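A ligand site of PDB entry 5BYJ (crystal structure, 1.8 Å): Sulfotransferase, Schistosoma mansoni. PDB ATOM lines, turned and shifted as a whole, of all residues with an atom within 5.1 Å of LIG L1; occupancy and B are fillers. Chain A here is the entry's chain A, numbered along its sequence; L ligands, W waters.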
ATOM      1  N   PRO A  18      29.235 -27.199   2.699  1.00  0.00           N
ATOM      2  CA  PRO A  18      28.206 -26.878   1.708  1.00  0.00           C
ATOM      3  C   PRO A  18      27.890 -25.374   1.670  1.00  0.00           C
ATOM      4  O   PRO A  18      28.058 -24.712   2.692  1.00  0.00           O
ATOM      5  CB  PRO A  18      26.982 -27.668   2.195  1.00  0.00           C
ATOM      6  CG  PRO A  18      27.319 -28.122   3.574  1.00  0.00           C
ATOM      7  CD  PRO A  18      28.798 -28.234   3.646  1.00  0.00           C
ATOM      8  N   HIS A  39      30.260 -35.283  -5.055  1.00  0.00           N
ATOM      9  CA  HIS A  39      29.507 -34.136  -4.545  1.00  0.00           C
ATOM     10  C   HIS A  39      28.189 -34.696  -4.026  1.00  0.00           C
ATOM     11  O   HIS A  39      27.816 -35.787  -4.435  1.00  0.00           O
ATOM     12  CB  HIS A  39      29.261 -33.110  -5.662  1.00  0.00           C
ATOM     13  CG  HIS A  39      28.640 -31.817  -5.189  1.00  0.00           C
ATOM     14  ND1 HIS A  39      27.272 -31.639  -5.095  1.00  0.00           N
ATOM     15  CD2 HIS A  39      29.197 -30.649  -4.812  1.00  0.00           C
ATOM     16  CE1 HIS A  39      27.032 -30.414  -4.660  1.00  0.00           C
ATOM     17  NE2 HIS A  39      28.180 -29.797  -4.483  1.00  0.00           N
ATOM     18  N   MET A  40      27.479 -33.982  -3.165  1.00  0.00           N
ATOM     19  CA  MET A  40      26.161 -34.472  -2.744  1.00  0.00           C
ATOM     20  C   MET A  40      25.246 -34.699  -3.963  1.00  0.00           C
ATOM     21  O   MET A  40      24.422 -35.610  -3.958  1.00  0.00           O
ATOM     22  CB  MET A  40      25.494 -33.529  -1.746  1.00  0.00           C
ATOM     23  CG  MET A  40      24.198 -34.084  -1.149  1.00  0.00           C
ATOM     24  SD  MET A  40      24.403 -35.610  -0.207  1.00  0.00           S
ATOM     25  CE  MET A  40      24.867 -34.980   1.407  1.00  0.00           C
ATOM     26  N   PHE A  41      25.405 -33.886  -4.992  1.00  0.00           N
ATOM     27  CA  PHE A  41      24.605 -34.047  -6.196  1.00  0.00           C
ATOM     28  C   PHE A  41      24.860 -35.410  -6.846  1.00  0.00           C
ATOM     29  O   PHE A  41      23.965 -35.968  -7.479  1.00  0.00           O
ATOM     30  CB  PHE A  41      24.892 -32.931  -7.204  1.00  0.00           C
ATOM     31  CG  PHE A  41      24.158 -31.666  -6.913  1.00  0.00           C
ATOM     32  CD1 PHE A  41      24.014 -31.207  -5.626  1.00  0.00           C
ATOM     33  CD2 PHE A  41      23.601 -30.923  -7.942  1.00  0.00           C
ATOM     34  CE1 PHE A  41      23.337 -30.040  -5.358  1.00  0.00           C
ATOM     35  CE2 PHE A  41      22.933 -29.753  -7.688  1.00  0.00           C
ATOM     36  CZ  PHE A  41      22.796 -29.313  -6.389  1.00  0.00           C
ATOM     37  N   ILE A  44      22.609 -37.766  -4.956  1.00  0.00           N
ATOM     38  CA  ILE A  44      21.197 -37.535  -5.230  1.00  0.00           C
ATOM     39  C   ILE A  44      20.762 -37.972  -6.621  1.00  0.00           C
ATOM     40  O   ILE A  44      19.685 -38.545  -6.797  1.00  0.00           O
ATOM     41  CB  ILE A  44      20.850 -36.050  -5.020  1.00  0.00           C
ATOM     42  CG1 ILE A  44      20.739 -35.778  -3.517  1.00  0.00           C
ATOM     43  CG2 ILE A  44      19.566 -35.673  -5.725  1.00  0.00           C
ATOM     44  CD1 ILE A  44      21.350 -34.494  -3.093  1.00  0.00           C
ATOM     45  N   ASP A  93      32.131 -31.216  -0.876  1.00  0.00           N
ATOM     46  CA  ASP A  93      30.793 -31.150  -0.260  1.00  0.00           C
ATOM     47  C   ASP A  93      30.600 -32.250   0.789  1.00  0.00           C
ATOM     48  O   ASP A  93      31.474 -33.112   0.978  1.00  0.00           O
ATOM     49  CB  ASP A  93      29.717 -31.243  -1.354  1.00  0.00           C
ATOM     50  CG  ASP A  93      28.350 -30.766  -0.919  1.00  0.00           C
ATOM     51  OD1 ASP A  93      28.239 -30.056   0.099  1.00  0.00           O
ATOM     52  OD2 ASP A  93      27.364 -31.110  -1.614  1.00  0.00           O
ATOM     53  N   LEU A  94      29.488 -32.179   1.512  1.00  0.00           N
ATOM     54  CA  LEU A  94      29.025 -33.307   2.323  1.00  0.00           C
ATOM     55  C   LEU A  94      28.743 -34.463   1.384  1.00  0.00           C
ATOM     56  O   LEU A  94      28.360 -34.236   0.231  1.00  0.00           O
ATOM     57  CB  LEU A  94      27.752 -32.960   3.092  1.00  0.00           C
ATOM     58  CG  LEU A  94      27.754 -31.796   4.078  1.00  0.00           C
ATOM     59  CD1 LEU A  94      26.342 -31.602   4.653  1.00  0.00           C
ATOM     60  CD2 LEU A  94      28.768 -32.060   5.182  1.00  0.00           C
ATOM     61  N   VAL A 129      18.543 -23.587   1.655  1.00  0.00           N
ATOM     62  CA  VAL A 129      18.749 -24.778   0.830  1.00  0.00           C
ATOM     63  C   VAL A 129      18.945 -26.088   1.608  1.00  0.00           C
ATOM     64  O   VAL A 129      18.345 -27.104   1.271  1.00  0.00           O
ATOM     65  CB  VAL A 129      19.965 -24.577  -0.082  1.00  0.00           C
ATOM     66  CG1 VAL A 129      20.250 -25.831  -0.933  1.00  0.00           C
ATOM     67  CG2 VAL A 129      19.755 -23.347  -0.970  1.00  0.00           C
ATOM     68  N   VAL A 130      19.799 -26.062   2.616  1.00  0.00           N
ATOM     69  CA  VAL A 130      20.272 -27.280   3.277  1.00  0.00           C
ATOM     70  C   VAL A 130      19.625 -27.504   4.638  1.00  0.00           C
ATOM     71  O   VAL A 130      19.281 -28.625   5.014  1.00  0.00           O
ATOM     72  CB  VAL A 130      21.804 -27.229   3.451  1.00  0.00           C
ATOM     73  CG1 VAL A 130      22.304 -28.319   4.412  1.00  0.00           C
ATOM     74  CG2 VAL A 130      22.482 -27.322   2.106  1.00  0.00           C
ATOM     75  N   LYS A 141       8.288 -27.091   1.687  1.00  0.00           N
ATOM     76  CA  LYS A 141       8.458 -27.087   0.233  1.00  0.00           C
ATOM     77  C   LYS A 141       9.676 -27.886  -0.159  1.00  0.00           C
ATOM     78  O   LYS A 141       9.643 -28.629  -1.136  1.00  0.00           O
ATOM     79  CB  LYS A 141       8.595 -25.652  -0.281  1.00  0.00           C
ATOM     80  CG  LYS A 141       7.356 -24.780  -0.076  1.00  0.00           C
ATOM     81  CD  LYS A 141       6.242 -25.168  -1.030  1.00  0.00           C
ATOM     82  CE  LYS A 141       5.213 -24.059  -1.149  1.00  0.00           C
ATOM     83  NZ  LYS A 141       5.847 -22.783  -1.595  1.00  0.00           N
ATOM     84  N   ILE A 142      10.775 -27.714   0.582  1.00  0.00           N
ATOM     85  CA  ILE A 142      11.964 -28.517   0.338  1.00  0.00           C
ATOM     86  C   ILE A 142      11.656 -30.013   0.450  1.00  0.00           C
ATOM     87  O   ILE A 142      12.052 -30.814  -0.400  1.00  0.00           O
ATOM     88  CB  ILE A 142      13.100 -28.149   1.322  1.00  0.00           C
ATOM     89  CG1 ILE A 142      13.604 -26.723   1.051  1.00  0.00           C
ATOM     90  CG2 ILE A 142      14.241 -29.133   1.232  1.00  0.00           C
ATOM     91  CD1 ILE A 142      14.713 -26.282   1.998  1.00  0.00           C
ATOM     92  N   GLY A 145       9.653 -31.253  -2.559  1.00  0.00           N
ATOM     93  CA  GLY A 145      10.462 -31.365  -3.752  1.00  0.00           C
ATOM     94  C   GLY A 145      11.424 -32.540  -3.631  1.00  0.00           C
ATOM     95  O   GLY A 145      11.662 -33.265  -4.604  1.00  0.00           O
ATOM     96  N   ASP A 146      11.969 -32.739  -2.440  1.00  0.00           N
ATOM     97  CA  ASP A 146      12.858 -33.863  -2.208  1.00  0.00           C
ATOM     98  C   ASP A 146      12.177 -35.212  -2.471  1.00  0.00           C
ATOM     99  O   ASP A 146      12.805 -36.129  -2.981  1.00  0.00           O
ATOM    100  CB  ASP A 146      13.413 -33.832  -0.795  1.00  0.00           C
ATOM    101  CG  ASP A 146      14.494 -32.797  -0.617  1.00  0.00           C
ATOM    102  OD1 ASP A 146      15.063 -32.363  -1.648  1.00  0.00           O
ATOM    103  OD2 ASP A 146      14.796 -32.430   0.531  1.00  0.00           O
ATOM    104  N   LEU A 149      12.356 -36.253  -5.917  1.00  0.00           N
ATOM    105  CA  LEU A 149      13.661 -36.808  -6.232  1.00  0.00           C
ATOM    106  C   LEU A 149      13.924 -38.189  -5.645  1.00  0.00           C
ATOM    107  O   LEU A 149      14.994 -38.751  -5.840  1.00  0.00           O
ATOM    108  CB  LEU A 149      14.766 -35.867  -5.747  1.00  0.00           C
ATOM    109  CG  LEU A 149      14.765 -34.480  -6.347  1.00  0.00           C
ATOM    110  CD1 LEU A 149      15.926 -33.676  -5.749  1.00  0.00           C
ATOM    111  CD2 LEU A 149      14.896 -34.607  -7.850  1.00  0.00           C
ATOM    112  N   LEU A 151      14.036 -38.819  -2.400  1.00  0.00           N
ATOM    113  CA  LEU A 151      14.780 -38.671  -1.143  1.00  0.00           C
ATOM    114  C   LEU A 151      13.863 -38.804   0.065  1.00  0.00           C
ATOM    115  O   LEU A 151      12.845 -38.114   0.156  1.00  0.00           O
ATOM    116  CB  LEU A 151      15.488 -37.319  -1.114  1.00  0.00           C
ATOM    117  CG  LEU A 151      16.407 -37.050  -2.294  1.00  0.00           C
ATOM    118  CD1 LEU A 151      16.951 -35.623  -2.246  1.00  0.00           C
ATOM    119  CD2 LEU A 151      17.541 -38.060  -2.291  1.00  0.00           C
ATOM    120  N   PHE A 155      17.976 -39.734   3.819  1.00  0.00           N
ATOM    121  CA  PHE A 155      18.779 -38.692   3.211  1.00  0.00           C
ATOM    122  C   PHE A 155      19.010 -37.546   4.179  1.00  0.00           C
ATOM    123  O   PHE A 155      20.134 -37.045   4.300  1.00  0.00           O
ATOM    124  CB  PHE A 155      18.115 -38.181   1.928  1.00  0.00           C
ATOM    125  CG  PHE A 155      18.842 -37.027   1.336  1.00  0.00           C
ATOM    126  CD1 PHE A 155      20.048 -37.216   0.678  1.00  0.00           C
ATOM    127  CD2 PHE A 155      18.344 -35.739   1.449  1.00  0.00           C
ATOM    128  CE1 PHE A 155      20.729 -36.131   0.134  1.00  0.00           C
ATOM    129  CE2 PHE A 155      19.025 -34.655   0.905  1.00  0.00           C
ATOM    130  CZ  PHE A 155      20.213 -34.861   0.246  1.00  0.00           C
ATOM    131  N   THR A 159      22.548 -36.076   5.815  1.00  0.00           N
ATOM    132  CA  THR A 159      22.947 -34.668   5.796  1.00  0.00           C
ATOM    133  C   THR A 159      23.277 -34.172   7.210  1.00  0.00           C
ATOM    134  O   THR A 159      24.347 -33.634   7.448  1.00  0.00           O
ATOM    135  CB  THR A 159      21.845 -33.784   5.208  1.00  0.00           C
ATOM    136  OG1 THR A 159      21.590 -34.177   3.857  1.00  0.00           O
ATOM    137  CG2 THR A 159      22.270 -32.330   5.268  1.00  0.00           C
ATOM    138  N   MET A 235      18.148 -22.835  -6.672  1.00  0.00           N
ATOM    139  CA  MET A 235      17.670 -23.996  -5.957  1.00  0.00           C
ATOM    140  C   MET A 235      16.196 -23.827  -5.581  1.00  0.00           C
ATOM    141  O   MET A 235      15.416 -24.780  -5.605  1.00  0.00           O
ATOM    142  CB  MET A 235      18.545 -24.241  -4.736  1.00  0.00           C
ATOM    143  CG  MET A 235      19.913 -24.725  -5.117  1.00  0.00           C
ATOM    144  SD  MET A 235      19.815 -26.410  -5.787  1.00  0.00           S
ATOM    145  CE  MET A 235      19.399 -27.308  -4.317  1.00  0.00           C
ATOM    146  N   LEU A 238      14.327 -24.659  -8.685  1.00  0.00           N
ATOM    147  CA  LEU A 238      14.293 -26.115  -8.883  1.00  0.00           C
ATOM    148  C   LEU A 238      13.256 -26.773  -7.990  1.00  0.00           C
ATOM    149  O   LEU A 238      12.496 -27.633  -8.442  1.00  0.00           O
ATOM    150  CB  LEU A 238      15.674 -26.719  -8.628  1.00  0.00           C
ATOM    151  CG  LEU A 238      15.746 -28.244  -8.571  1.00  0.00           C
ATOM    152  CD1 LEU A 238      15.323 -28.841  -9.905  1.00  0.00           C
ATOM    153  CD2 LEU A 238      17.157 -28.704  -8.191  1.00  0.00           C
ATOM    154  N   THR A 239      13.235 -26.386  -6.719  1.00  0.00           N
ATOM    155  CA  THR A 239      12.258 -26.917  -5.772  1.00  0.00           C
ATOM    156  C   THR A 239      10.825 -26.660  -6.247  1.00  0.00           C
ATOM    157  O   THR A 239       9.995 -27.558  -6.243  1.00  0.00           O
ATOM    158  CB  THR A 239      12.434 -26.287  -4.385  1.00  0.00           C
ATOM    159  OG1 THR A 239      13.741 -26.568  -3.896  1.00  0.00           O
ATOM    160  CG2 THR A 239      11.397 -26.832  -3.395  1.00  0.00           C
ATOM    161  N   LEU A 242      10.011 -28.771  -9.275  1.00  0.00           N
ATOM    162  CA  LEU A 242       9.827 -30.185  -8.930  1.00  0.00           C
ATOM    163  C   LEU A 242       8.421 -30.401  -8.390  1.00  0.00           C
ATOM    164  O   LEU A 242       7.753 -31.402  -8.709  1.00  0.00           O
ATOM    165  CB  LEU A 242      10.870 -30.649  -7.896  1.00  0.00           C
ATOM    166  CG  LEU A 242      12.277 -30.877  -8.442  1.00  0.00           C
ATOM    167  CD1 LEU A 242      13.308 -30.997  -7.306  1.00  0.00           C
ATOM    168  CD2 LEU A 242      12.330 -32.123  -9.314  1.00  0.00           C
HETATM  169  C1  LIG L   1      19.567 -31.592  -3.692  1.00  0.00           C
HETATM  170  C2  LIG L   1      20.625 -30.528  -3.394  1.00  0.00           C
HETATM  171  C3  LIG L   1      21.105 -30.655  -2.088  1.00  0.00           C
HETATM  172  C4  LIG L   1      22.441 -30.337  -1.780  1.00  0.00           C
HETATM  173  C5  LIG L   1      22.945 -30.453  -0.483  1.00  0.00           C
HETATM  174  C6  LIG L   1      24.287 -30.124  -0.211  1.00  0.00           C
HETATM  175  O1  LIG L   1      25.098 -30.108  -1.407  1.00  0.00           O
HETATM  176  C7  LIG L   1      22.038 -30.884   0.508  1.00  0.00           C
HETATM  177  N1  LIG L   1      22.386 -31.032   1.797  1.00  0.00           N
HETATM  178  O2  LIG L   1      21.306 -30.926   2.717  1.00  0.00           O
HETATM  179  O3  LIG L   1      23.781 -31.436   2.247  1.00  0.00           O
HETATM  180  C8  LIG L   1      20.714 -31.180   0.214  1.00  0.00           C
HETATM  181  C9  LIG L   1      20.243 -31.064  -1.083  1.00  0.00           C
HETATM  182  N2  LIG L   1      18.899 -31.401  -1.353  1.00  0.00           N
HETATM  183  C10 LIG L   1      18.404 -31.433  -2.743  1.00  0.00           C
HETATM  184  C11 LIG L   1      17.696 -30.148  -3.095  1.00  0.00           C
HETATM  185  N3  LIG L   1      16.378 -30.063  -2.467  1.00  0.00           N
HETATM  186  C12 LIG L   1      15.403 -29.970  -3.563  1.00  0.00           C
HETATM  187  C13 LIG L   1      15.833 -28.909  -4.576  1.00  0.00           C
HETATM  188  C14 LIG L   1      13.994 -29.664  -3.009  1.00  0.00           C
HETATM  189  P1  LG2 L   2      24.192 -18.330  -2.609  1.00  0.00           P
HETATM  190  O1  LG2 L   2      24.428 -17.221  -1.614  1.00  0.00           O
HETATM  191  O2  LG2 L   2      23.196 -19.361  -2.089  1.00  0.00           O
HETATM  192  O3  LG2 L   2      23.697 -17.806  -3.938  1.00  0.00           O
HETATM  193  P2  LG2 L   2      27.441 -24.847  -3.057  1.00  0.00           P
HETATM  194  O4  LG2 L   2      28.625 -25.242  -2.210  1.00  0.00           O
HETATM  195  O5  LG2 L   2      27.562 -25.304  -4.477  1.00  0.00           O
HETATM  196  O6  LG2 L   2      26.126 -25.269  -2.425  1.00  0.00           O
HETATM  197  O7  LG2 L   2      27.548 -23.253  -3.025  1.00  0.00           O
HETATM  198  C1  LG2 L   2      26.613 -22.445  -3.750  1.00  0.00           C
HETATM  199  C2  LG2 L   2      26.816 -21.012  -3.336  1.00  0.00           C
HETATM  200  O8  LG2 L   2      28.063 -20.497  -3.899  1.00  0.00           O
HETATM  201  C3  LG2 L   2      25.738 -20.115  -3.850  1.00  0.00           C
HETATM  202  O9  LG2 L   2      25.615 -19.015  -2.918  1.00  0.00           O
HETATM  203  C4  LG2 L   2      26.304 -19.654  -5.141  1.00  0.00           C
HETATM  204  O10 LG2 L   2      25.688 -18.458  -5.602  1.00  0.00           O
HETATM  205  C5  LG2 L   2      27.733 -19.408  -4.797  1.00  0.00           C
HETATM  206  N1  LG2 L   2      28.614 -19.474  -5.904  1.00  0.00           N
HETATM  207  C6  LG2 L   2      28.871 -20.559  -6.637  1.00  0.00           C
HETATM  208  N2  LG2 L   2      29.744 -20.271  -7.602  1.00  0.00           N
HETATM  209  C7  LG2 L   2      30.071 -18.945  -7.487  1.00  0.00           C
HETATM  210  C8  LG2 L   2      30.943 -18.059  -8.197  1.00  0.00           C
HETATM  211  N3  LG2 L   2      31.697 -18.515  -9.289  1.00  0.00           N
HETATM  212  N4  LG2 L   2      31.021 -16.777  -7.800  1.00  0.00           N
HETATM  213  C9  LG2 L   2      30.321 -16.342  -6.765  1.00  0.00           C
HETATM  214  N5  LG2 L   2      29.491 -17.127  -6.076  1.00  0.00           N
HETATM  215  C10 LG2 L   2      29.345 -18.435  -6.403  1.00  0.00           C
HETATM  216  O   HOH W   1      17.469 -31.061   0.717  1.00  0.00           O
HETATM  217  O   HOH W   2      23.910 -27.539  -1.991  1.00  0.00           O
HETATM  218  O   HOH W   3      17.162 -27.681  -1.196  1.00  0.00           O
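The side-chain carboxylate (OD1) of Asp 146 lies within salt-bridge range of a nitrogen (N3) of LIG L1 (2.8 Å). O2 of LIG L1 lies close to OG1 of Thr 159 (3.5 Å). OD2 of Asp 93 sits at hydrogen-bond distance from O1 of LIG L1.
The side-chain hydroxyl of Thr 239 is in hydrogen-bond range of the backbone carbonyl oxygen of Met 235. The backbone carbonyl oxygen (O) of Asp 146 lies within hydrogen-bond range of the backbone NH (N) of Leu 151, 3.0 Å away. The side-chain carboxylate (OD2) of Asp 93 lies close to the backbone NH (N) of Met 40 (3.3 Å). A ring nitrogen (NE2) of His 39 lies close to the side-chain carboxylate of Asp 93 (3.3 Å). ND1 of His 39 lies within hydrogen-bond range of N of Phe 41, at 2.9 Å. The backbone carbonyl oxygen (O) of Phe 155 is in hydrogen-bond range of the side-chain hydroxyl (OG1) of Thr 159 (3.2 Å).
Residues that only touch LIG L1: His 39 (3.8 Å), Met 40 (3.5 Å), Phe 41 (3.4 Å), Ile 44 (3.5 Å), Leu 94 (3.5 Å), Val 130 (3.3 Å), Ile 142 (3.4 Å), Gly 145 (3.9 Å), Phe 155 (3.7 Å), Met 235 (3.5 Å), Leu 238 (3.9 Å) and Thr 239 (3.2 Å). Hydrophobic or aromatic side chains that line LIG L1: His 39, Met 40, Phe 41, Ile 44, Leu 94, Val 130, Phe 155, Met 235 and Leu 238. 15 residues have an atom within 4 Å of LIG L1: His 39, Met 40, Phe 41, Ile 44, Asp 93, Leu 94, Val 130, Ile 142, Gly 145, Asp 146, Phe 155, Thr 159, Met 235, Leu 238 and Thr 239. Along chain A the residues within 4 Å of LIG L1 span positions 39 to 239. The nearest printed residue that does not touch LIG L1 is Leu 242 (4.3 Å).
Water W1 lies within hydrogen-bond range of N2 of LIG L1 (2.5 Å) and OD2 of Asp 146 (3.0 Å). Water W3 bridges the backbone carbonyl oxygen (O) of Val 129 and a nitrogen (N3) of LIG L1. Water W2 bridges O1 of LIG L1 (2.9 Å) and O6 of LG2 L2 (3.2 Å).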
